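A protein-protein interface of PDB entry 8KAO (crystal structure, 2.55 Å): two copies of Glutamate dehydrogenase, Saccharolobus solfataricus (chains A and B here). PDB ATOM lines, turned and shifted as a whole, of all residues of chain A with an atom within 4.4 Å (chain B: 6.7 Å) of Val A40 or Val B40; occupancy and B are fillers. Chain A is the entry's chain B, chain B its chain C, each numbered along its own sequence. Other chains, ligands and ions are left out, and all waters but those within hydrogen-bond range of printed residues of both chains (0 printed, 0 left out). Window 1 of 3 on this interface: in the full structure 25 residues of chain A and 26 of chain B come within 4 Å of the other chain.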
ATOM      1  N   PRO A  37     -13.467 -31.506   6.163  1.00  0.00           N
ATOM      2  CA  PRO A  37     -14.317 -31.382   7.342  1.00  0.00           C
ATOM      3  C   PRO A  37     -15.526 -30.508   7.043  1.00  0.00           C
ATOM      4  O   PRO A  37     -15.475 -29.650   6.155  1.00  0.00           O
ATOM      5  CB  PRO A  37     -13.375 -30.748   8.367  1.00  0.00           C
ATOM      6  CG  PRO A  37     -12.474 -29.894   7.535  1.00  0.00           C
ATOM      7  CD  PRO A  37     -12.221 -30.737   6.311  1.00  0.00           C
ATOM      8  N   ARG A  39     -17.095 -28.412   9.182  1.00  0.00           N
ATOM      9  CA  ARG A  39     -16.794 -27.088   9.666  1.00  0.00           C
ATOM     10  C   ARG A  39     -15.502 -27.140  10.466  1.00  0.00           C
ATOM     11  O   ARG A  39     -15.211 -28.148  11.109  1.00  0.00           O
ATOM     12  CB  ARG A  39     -17.948 -26.580  10.521  1.00  0.00           C
ATOM     13  CG  ARG A  39     -17.759 -25.122  11.041  1.00  0.00           C
ATOM     14  CD  ARG A  39     -19.063 -24.630  11.729  1.00  0.00           C
ATOM     15  NE  ARG A  39     -19.812 -25.775  12.234  1.00  0.00           N
ATOM     16  CZ  ARG A  39     -20.924 -26.260  11.679  1.00  0.00           C
ATOM     17  NH1 ARG A  39     -21.540 -25.575  10.736  1.00  0.00           N
ATOM     18  NH2 ARG A  39     -21.444 -27.404  12.112  1.00  0.00           N
ATOM     19  N   VAL A  40     -14.752 -26.031  10.415  1.00  0.00           N
ATOM     20  CA  VAL A  40     -13.588 -25.823  11.258  1.00  0.00           C
ATOM     21  C   VAL A  40     -13.620 -24.369  11.722  1.00  0.00           C
ATOM     22  O   VAL A  40     -13.868 -23.465  10.924  1.00  0.00           O
ATOM     23  CB  VAL A  40     -12.267 -26.155  10.529  1.00  0.00           C
ATOM     24  CG1 VAL A  40     -12.092 -27.649  10.293  1.00  0.00           C
ATOM     25  CG2 VAL A  40     -12.148 -25.456   9.186  1.00  0.00           C
ATOM     26  N   MET A  41     -13.370 -24.137  13.009  1.00  0.00           N
ATOM     27  CA  MET A  41     -13.223 -22.762  13.442  1.00  0.00           C
ATOM     28  C   MET A  41     -11.888 -22.556  14.144  1.00  0.00           C
ATOM     29  O   MET A  41     -11.349 -23.452  14.800  1.00  0.00           O
ATOM     30  CB  MET A  41     -14.360 -22.301  14.360  1.00  0.00           C
ATOM     31  CG  MET A  41     -15.433 -23.329  14.579  1.00  0.00           C
ATOM     32  SD  MET A  41     -16.677 -22.770  15.749  1.00  0.00           S
ATOM     33  CE  MET A  41     -17.240 -24.383  16.289  1.00  0.00           C
ATOM     34  N   GLN A  42     -11.397 -21.323  13.987  1.00  0.00           N
ATOM     35  CA  GLN A  42     -10.183 -20.866  14.624  1.00  0.00           C
ATOM     36  C   GLN A  42     -10.506 -19.592  15.394  1.00  0.00           C
ATOM     37  O   GLN A  42     -11.254 -18.749  14.894  1.00  0.00           O
ATOM     38  CB  GLN A  42      -9.111 -20.611  13.569  1.00  0.00           C
ATOM     39  CG  GLN A  42      -8.046 -19.631  14.026  1.00  0.00           C
ATOM     40  CD  GLN A  42      -7.091 -19.320  12.911  1.00  0.00           C
ATOM     41  OE1 GLN A  42      -6.439 -20.212  12.375  1.00  0.00           O
ATOM     42  NE2 GLN A  42      -7.043 -18.052  12.536  1.00  0.00           N
ATOM     43  N   ARG A  61     -11.186 -25.829  16.401  1.00  0.00           N
ATOM     44  CA  ARG A  61     -12.119 -26.934  16.563  1.00  0.00           C
ATOM     45  C   ARG A  61     -12.460 -27.396  15.160  1.00  0.00           C
ATOM     46  O   ARG A  61     -13.069 -26.632  14.405  1.00  0.00           O
ATOM     47  CB  ARG A  61     -13.408 -26.521  17.291  1.00  0.00           C
ATOM     48  CG  ARG A  61     -14.339 -27.672  17.658  1.00  0.00           C
ATOM     49  CD  ARG A  61     -13.739 -28.623  18.687  1.00  0.00           C
ATOM     50  NE  ARG A  61     -14.582 -29.783  18.941  1.00  0.00           N
ATOM     51  CZ  ARG A  61     -14.192 -30.852  19.639  1.00  0.00           C
ATOM     52  NH1 ARG A  61     -12.999 -30.869  20.218  1.00  0.00           N
ATOM     53  NH2 ARG A  61     -14.988 -31.907  19.755  1.00  0.00           N
ATOM     54  N   SER A  62     -12.006 -28.612  14.818  1.00  0.00           N
ATOM     55  CA  SER A  62     -12.403 -29.243  13.574  1.00  0.00           C
ATOM     56  C   SER A  62     -13.532 -30.231  13.851  1.00  0.00           C
ATOM     57  O   SER A  62     -13.426 -31.113  14.707  1.00  0.00           O
ATOM     58  CB  SER A  62     -11.248 -29.875  12.870  1.00  0.00           C
ATOM     59  OG  SER A  62     -11.693 -30.590  11.720  1.00  0.00           O
ATOM     60  N   ILE A  87      -7.504 -31.016  12.229  1.00  0.00           N
ATOM     61  CA  ILE A  87      -8.378 -31.588  11.213  1.00  0.00           C
ATOM     62  C   ILE A  87      -8.129 -33.081  11.105  1.00  0.00           C
ATOM     63  O   ILE A  87      -9.057 -33.869  11.124  1.00  0.00           O
ATOM     64  CB  ILE A  87      -8.191 -30.916   9.846  1.00  0.00           C
ATOM     65  CG1 ILE A  87      -8.599 -29.442   9.879  1.00  0.00           C
ATOM     66  CG2 ILE A  87      -8.976 -31.678   8.803  1.00  0.00           C
ATOM     67  CD1 ILE A  87      -8.492 -28.731   8.546  1.00  0.00           C
ATOM     68  N   PRO B  37      -7.805 -12.357  13.482  1.00  0.00           N
ATOM     69  CA  PRO B  37      -9.265 -12.357  13.505  1.00  0.00           C
ATOM     70  C   PRO B  37      -9.718 -13.050  14.784  1.00  0.00           C
ATOM     71  O   PRO B  37      -9.074 -14.005  15.218  1.00  0.00           O
ATOM     72  CB  PRO B  37      -9.622 -13.151  12.240  1.00  0.00           C
ATOM     73  CG  PRO B  37      -8.491 -14.157  12.134  1.00  0.00           C
ATOM     74  CD  PRO B  37      -7.260 -13.390  12.583  1.00  0.00           C
ATOM     75  N   GLU B  38     -10.815 -12.563  15.380  1.00  0.00           N
ATOM     76  CA  GLU B  38     -11.351 -13.174  16.583  1.00  0.00           C
ATOM     77  C   GLU B  38     -11.827 -14.586  16.264  1.00  0.00           C
ATOM     78  O   GLU B  38     -11.601 -15.512  17.054  1.00  0.00           O
ATOM     79  CB  GLU B  38     -12.497 -12.340  17.154  1.00  0.00           C
ATOM     80  CG  GLU B  38     -12.037 -10.989  17.681  1.00  0.00           C
ATOM     81  CD  GLU B  38     -13.147  -9.981  17.910  1.00  0.00           C
ATOM     82  OE1 GLU B  38     -14.308 -10.327  17.670  1.00  0.00           O
ATOM     83  OE2 GLU B  38     -12.836  -8.841  18.268  1.00  0.00           O
ATOM     84  N   ARG B  39     -12.484 -14.745  15.103  1.00  0.00           N
ATOM     85  CA  ARG B  39     -13.009 -16.049  14.733  1.00  0.00           C
ATOM     86  C   ARG B  39     -13.030 -16.216  13.220  1.00  0.00           C
ATOM     87  O   ARG B  39     -13.418 -15.326  12.474  1.00  0.00           O
ATOM     88  CB  ARG B  39     -14.427 -16.258  15.279  1.00  0.00           C
ATOM     89  CG  ARG B  39     -14.981 -17.703  15.065  1.00  0.00           C
ATOM     90  CD  ARG B  39     -16.317 -17.829  15.842  1.00  0.00           C
ATOM     91  NE  ARG B  39     -16.955 -16.526  16.011  1.00  0.00           N
ATOM     92  CZ  ARG B  39     -17.187 -15.946  17.182  1.00  0.00           C
ATOM     93  NH1 ARG B  39     -16.983 -16.616  18.316  1.00  0.00           N
ATOM     94  NH2 ARG B  39     -17.679 -14.713  17.211  1.00  0.00           N
ATOM     95  N   VAL B  40     -12.662 -17.417  12.790  1.00  0.00           N
ATOM     96  CA  VAL B  40     -12.718 -17.783  11.388  1.00  0.00           C
ATOM     97  C   VAL B  40     -13.388 -19.152  11.287  1.00  0.00           C
ATOM     98  O   VAL B  40     -13.018 -20.094  12.000  1.00  0.00           O
ATOM     99  CB  VAL B  40     -11.324 -17.784  10.735  1.00  0.00           C
ATOM    100  CG1 VAL B  40     -11.126 -16.613   9.799  1.00  0.00           C
ATOM    101  CG2 VAL B  40     -10.218 -17.761  11.768  1.00  0.00           C
ATOM    102  N   MET B  41     -14.380 -19.240  10.402  1.00  0.00           N
ATOM    103  CA  MET B  41     -14.981 -20.517  10.063  1.00  0.00           C
ATOM    104  C   MET B  41     -14.670 -20.854   8.610  1.00  0.00           C
ATOM    105  O   MET B  41     -14.750 -19.981   7.745  1.00  0.00           O
ATOM    106  CB  MET B  41     -16.501 -20.462  10.242  1.00  0.00           C
ATOM    107  CG  MET B  41     -16.899 -20.089  11.660  1.00  0.00           C
ATOM    108  SD  MET B  41     -18.672 -19.972  11.844  1.00  0.00           S
ATOM    109  CE  MET B  41     -18.886 -18.226  11.472  1.00  0.00           C
ATOM    110  N   GLN B  42     -14.287 -22.119   8.384  1.00  0.00           N
ATOM    111  CA  GLN B  42     -14.275 -22.723   7.067  1.00  0.00           C
ATOM    112  C   GLN B  42     -15.343 -23.807   7.053  1.00  0.00           C
ATOM    113  O   GLN B  42     -15.482 -24.503   8.054  1.00  0.00           O
ATOM    114  CB  GLN B  42     -12.892 -23.310   6.798  1.00  0.00           C
ATOM    115  CG  GLN B  42     -12.909 -24.479   5.824  1.00  0.00           C
ATOM    116  CD  GLN B  42     -11.516 -25.001   5.604  1.00  0.00           C
ATOM    117  OE1 GLN B  42     -10.628 -24.263   5.189  1.00  0.00           O
ATOM    118  NE2 GLN B  42     -11.310 -26.266   5.929  1.00  0.00           N
ATOM    119  N   VAL B  43     -16.063 -23.959   5.926  1.00  0.00           N
ATOM    120  CA  VAL B  43     -17.160 -24.920   5.802  1.00  0.00           C
ATOM    121  C   VAL B  43     -17.101 -25.616   4.448  1.00  0.00           C
ATOM    122  O   VAL B  43     -16.694 -25.015   3.466  1.00  0.00           O
ATOM    123  CB  VAL B  43     -18.526 -24.240   5.964  1.00  0.00           C
ATOM    124  CG1 VAL B  43     -18.757 -23.827   7.411  1.00  0.00           C
ATOM    125  CG2 VAL B  43     -18.680 -23.066   5.009  1.00  0.00           C
ATOM    126  N   LYS B  44     -17.535 -26.874   4.409  1.00  0.00           N
ATOM    127  CA  LYS B  44     -17.520 -27.673   3.191  1.00  0.00           C
ATOM    128  C   LYS B  44     -18.918 -27.683   2.591  1.00  0.00           C
ATOM    129  O   LYS B  44     -19.875 -28.072   3.272  1.00  0.00           O
ATOM    130  CB  LYS B  44     -17.114 -29.112   3.513  1.00  0.00           C
ATOM    131  CG  LYS B  44     -17.423 -30.132   2.431  1.00  0.00           C
ATOM    132  CD  LYS B  44     -17.173 -31.544   2.884  1.00  0.00           C
ATOM    133  CE  LYS B  44     -17.967 -31.884   4.129  1.00  0.00           C
ATOM    134  NZ  LYS B  44     -17.757 -33.298   4.518  1.00  0.00           N
ATOM    135  N   TRP B  60     -15.254 -19.590   3.523  1.00  0.00           N
ATOM    136  CA  TRP B  60     -14.780 -19.040   4.781  1.00  0.00           C
ATOM    137  C   TRP B  60     -15.652 -17.852   5.172  1.00  0.00           C
ATOM    138  O   TRP B  60     -16.211 -17.141   4.312  1.00  0.00           O
ATOM    139  CB  TRP B  60     -13.313 -18.588   4.701  1.00  0.00           C
ATOM    140  CG  TRP B  60     -12.377 -19.664   4.258  1.00  0.00           C
ATOM    141  CD1 TRP B  60     -11.648 -20.477   5.064  1.00  0.00           C
ATOM    142  CD2 TRP B  60     -12.086 -20.049   2.906  1.00  0.00           C
ATOM    143  NE1 TRP B  60     -10.947 -21.371   4.311  1.00  0.00           N
ATOM    144  CE2 TRP B  60     -11.180 -21.126   2.986  1.00  0.00           C
ATOM    145  CE3 TRP B  60     -12.503 -19.598   1.646  1.00  0.00           C
ATOM    146  CZ2 TRP B  60     -10.696 -21.775   1.854  1.00  0.00           C
ATOM    147  CZ3 TRP B  60     -12.025 -20.237   0.524  1.00  0.00           C
ATOM    148  CH2 TRP B  60     -11.130 -21.306   0.633  1.00  0.00           C
ATOM    149  N   ARG B  61     -15.755 -17.675   6.497  1.00  0.00           N
ATOM    150  CA  ARG B  61     -16.252 -16.441   7.070  1.00  0.00           C
ATOM    151  C   ARG B  61     -15.226 -16.076   8.126  1.00  0.00           C
ATOM    152  O   ARG B  61     -14.905 -16.906   8.976  1.00  0.00           O
ATOM    153  CB  ARG B  61     -17.681 -16.583   7.622  1.00  0.00           C
ATOM    154  CG  ARG B  61     -18.357 -15.267   8.012  1.00  0.00           C
ATOM    155  CD  ARG B  61     -18.661 -14.271   6.888  1.00  0.00           C
ATOM    156  NE  ARG B  61     -19.035 -12.958   7.420  1.00  0.00           N
ATOM    157  CZ  ARG B  61     -19.355 -11.876   6.702  1.00  0.00           C
ATOM    158  NH1 ARG B  61     -19.236 -11.849   5.383  1.00  0.00           N
ATOM    159  NH2 ARG B  61     -19.790 -10.799   7.321  1.00  0.00           N
ATOM    160  N   SER B  62     -14.652 -14.877   7.955  1.00  0.00           N
ATOM    161  CA  SER B  62     -13.653 -14.340   8.861  1.00  0.00           C
ATOM    162  C   SER B  62     -14.281 -13.163   9.590  1.00  0.00           C
ATOM    163  O   SER B  62     -14.765 -12.221   8.953  1.00  0.00           O
ATOM    164  CB  SER B  62     -12.385 -13.934   8.177  1.00  0.00           C
ATOM    165  OG  SER B  62     -11.555 -13.213   9.084  1.00  0.00           O
ATOM    166  N   GLN B  63     -14.266 -13.302  10.922  1.00  0.00           N
ATOM    167  CA  GLN B  63     -14.880 -12.402  11.866  1.00  0.00           C
ATOM    168  C   GLN B  63     -13.702 -11.800  12.615  1.00  0.00           C
ATOM    169  O   GLN B  63     -13.145 -12.431  13.522  1.00  0.00           O
ATOM    170  CB  GLN B  63     -15.864 -13.210  12.720  1.00  0.00           C
ATOM    171  CG  GLN B  63     -17.013 -13.814  11.912  1.00  0.00           C
ATOM    172  CD  GLN B  63     -18.016 -14.618  12.701  1.00  0.00           C
ATOM    173  OE1 GLN B  63     -17.714 -15.135  13.765  1.00  0.00           O
ATOM    174  NE2 GLN B  63     -19.234 -14.735  12.187  1.00  0.00           N
ATOM    175  N   GLN B  83      -8.447 -18.679   2.402  1.00  0.00           N
ATOM    176  CA  GLN B  83      -8.725 -18.340   3.793  1.00  0.00           C
ATOM    177  C   GLN B  83      -8.023 -17.027   4.086  1.00  0.00           C
ATOM    178  O   GLN B  83      -8.638 -16.096   4.595  1.00  0.00           O
ATOM    179  CB  GLN B  83      -8.229 -19.446   4.729  1.00  0.00           C
ATOM    180  CG  GLN B  83      -8.572 -19.274   6.195  1.00  0.00           C
ATOM    181  CD  GLN B  83      -7.537 -19.964   7.052  1.00  0.00           C
ATOM    182  OE1 GLN B  83      -7.786 -20.998   7.663  1.00  0.00           O
ATOM    183  NE2 GLN B  83      -6.328 -19.417   7.064  1.00  0.00           N
ATOM    184  N   VAL B  86      -9.643 -13.734   2.583  1.00  0.00           N
ATOM    185  CA  VAL B  86     -10.879 -13.327   3.249  1.00  0.00           C
ATOM    186  C   VAL B  86     -10.568 -12.768   4.644  1.00  0.00           C
ATOM    187  O   VAL B  86     -11.108 -11.737   5.038  1.00  0.00           O
ATOM    188  CB  VAL B  86     -11.953 -14.433   3.266  1.00  0.00           C
ATOM    189  CG1 VAL B  86     -11.404 -15.776   3.677  1.00  0.00           C
ATOM    190  CG2 VAL B  86     -13.136 -14.078   4.159  1.00  0.00           C
ATOM    191  N   ILE B  87      -9.638 -13.380   5.371  1.00  0.00           N
ATOM    192  CA  ILE B  87      -9.162 -12.802   6.617  1.00  0.00           C
ATOM    193  C   ILE B  87      -8.589 -11.406   6.379  1.00  0.00           C
ATOM    194  O   ILE B  87      -8.782 -10.523   7.203  1.00  0.00           O
ATOM    195  CB  ILE B  87      -8.103 -13.700   7.277  1.00  0.00           C
ATOM    196  CG1 ILE B  87      -8.685 -15.038   7.737  1.00  0.00           C
ATOM    197  CG2 ILE B  87      -7.425 -12.963   8.430  1.00  0.00           C
ATOM    198  CD1 ILE B  87      -7.638 -15.958   8.325  1.00  0.00           C
ATOM    199  N   SER B  90     -11.313  -9.043   5.847  1.00  0.00           N
ATOM    200  CA  SER B  90     -11.839  -8.814   7.188  1.00  0.00           C
ATOM    201  C   SER B  90     -11.203  -7.570   7.782  1.00  0.00           C
ATOM    202  O   SER B  90     -11.893  -6.711   8.315  1.00  0.00           O
ATOM    203  CB  SER B  90     -11.521  -9.957   8.120  1.00  0.00           C
ATOM    204  OG  SER B  90     -12.345 -11.076   7.904  1.00  0.00           O
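O of Val A40 is in hydrogen-bond range of N of Gln B42 (2.9 Å). The backbone NH (N) of Gln A42 sits at hydrogen-bond distance from the backbone carbonyl oxygen (O) of Val B40 (2.8 Å).
The backbone carbonyl oxygen of Met A41 is in hydrogen-bond range of the backbone NH of Arg A61, at 2.9 Å. O of Gln B63 sits at hydrogen-bond distance from N of Glu B38. The backbone NH of Gln B63 is in hydrogen-bond range of the backbone carbonyl oxygen of Arg B39. N of Met B41 sits at hydrogen-bond distance from O of Arg B61 (2.8 Å). The indole nitrogen (NE1) of Trp B60 is in hydrogen-bond range of the side-chain amide oxygen (OE1) of Gln B42.
Among the printed residues, pairs that only touch across the chains: Pro A37 with Lys B44, Arg A39 with Gln B42, Arg A39 with Val B43, Val A40 with Val B40, Val A40 with Met B41, Met A41 with Val B40, Gln A42 with Glu B38 and Gln A42 with Arg B39.
Of chain B, only Val B40, Met B41 and Gln B42 come within 4 Å of Val A40. Val B40 touches three residues of chain A. Of the printed residues of chain A, Lys B44 touches Pro A37. Of the printed residues of chain A, Val B43 touches Arg A39 (3.98 Å). Printed residues of chain A within 4 Å of Glu B38: Gln A42 (3.9 Å). Printed residues of chain A within 4 Å of Arg B39: Gln A42. Printed residues of chain B within 4 Å of Gln A42: Glu B38, Arg B39 and Val B40. The nearest residue of chain B that does not touch Val A40 is Val B43 (5.1 Å). The nearest printed residue of chain A that does not touch Val B40 is Arg A61 (7.0 Å).
Hydrophobic or aromatic side chains of chain B that line the printed part of chain A: Val B40 and Val B43. Along chain B the printed residues that touch a printed residue of chain A span positions 38 to 44. Of the 8 printed residues of chain A, 5 touch a printed residue of chain B. Printed residues of chain A that touch a printed residue of chain B: Pro A37, Arg A39, Val A40, Met A41 and Gln A42. Hydrophobic or aromatic side chains of chain A within 4 Å of the printed part of chain B: Val A40 and Met A41. Among the printed residues, 10 pairs touch across the chains. Among the printed residues, no Asp or Glu carboxylate lies within 4 Å of a Lys or Arg side-chain nitrogen of the other chain.
Arg A39 touches Gln B42, and with the chains exchanged Gln A42 touches Arg B39. Val B40 touches its own counterpart, Val A40. Val A40 touches Met B41, and with the chains exchanged Met A41 touches Val B40. Val A40 touches Gln B42, and with the chains exchanged Gln A42 touches Val B40. 8 positions are printed for both chains. Of the 10 pairs that touch across the chains among the printed residues, 7 have their exchanged pair printed and touching as well.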
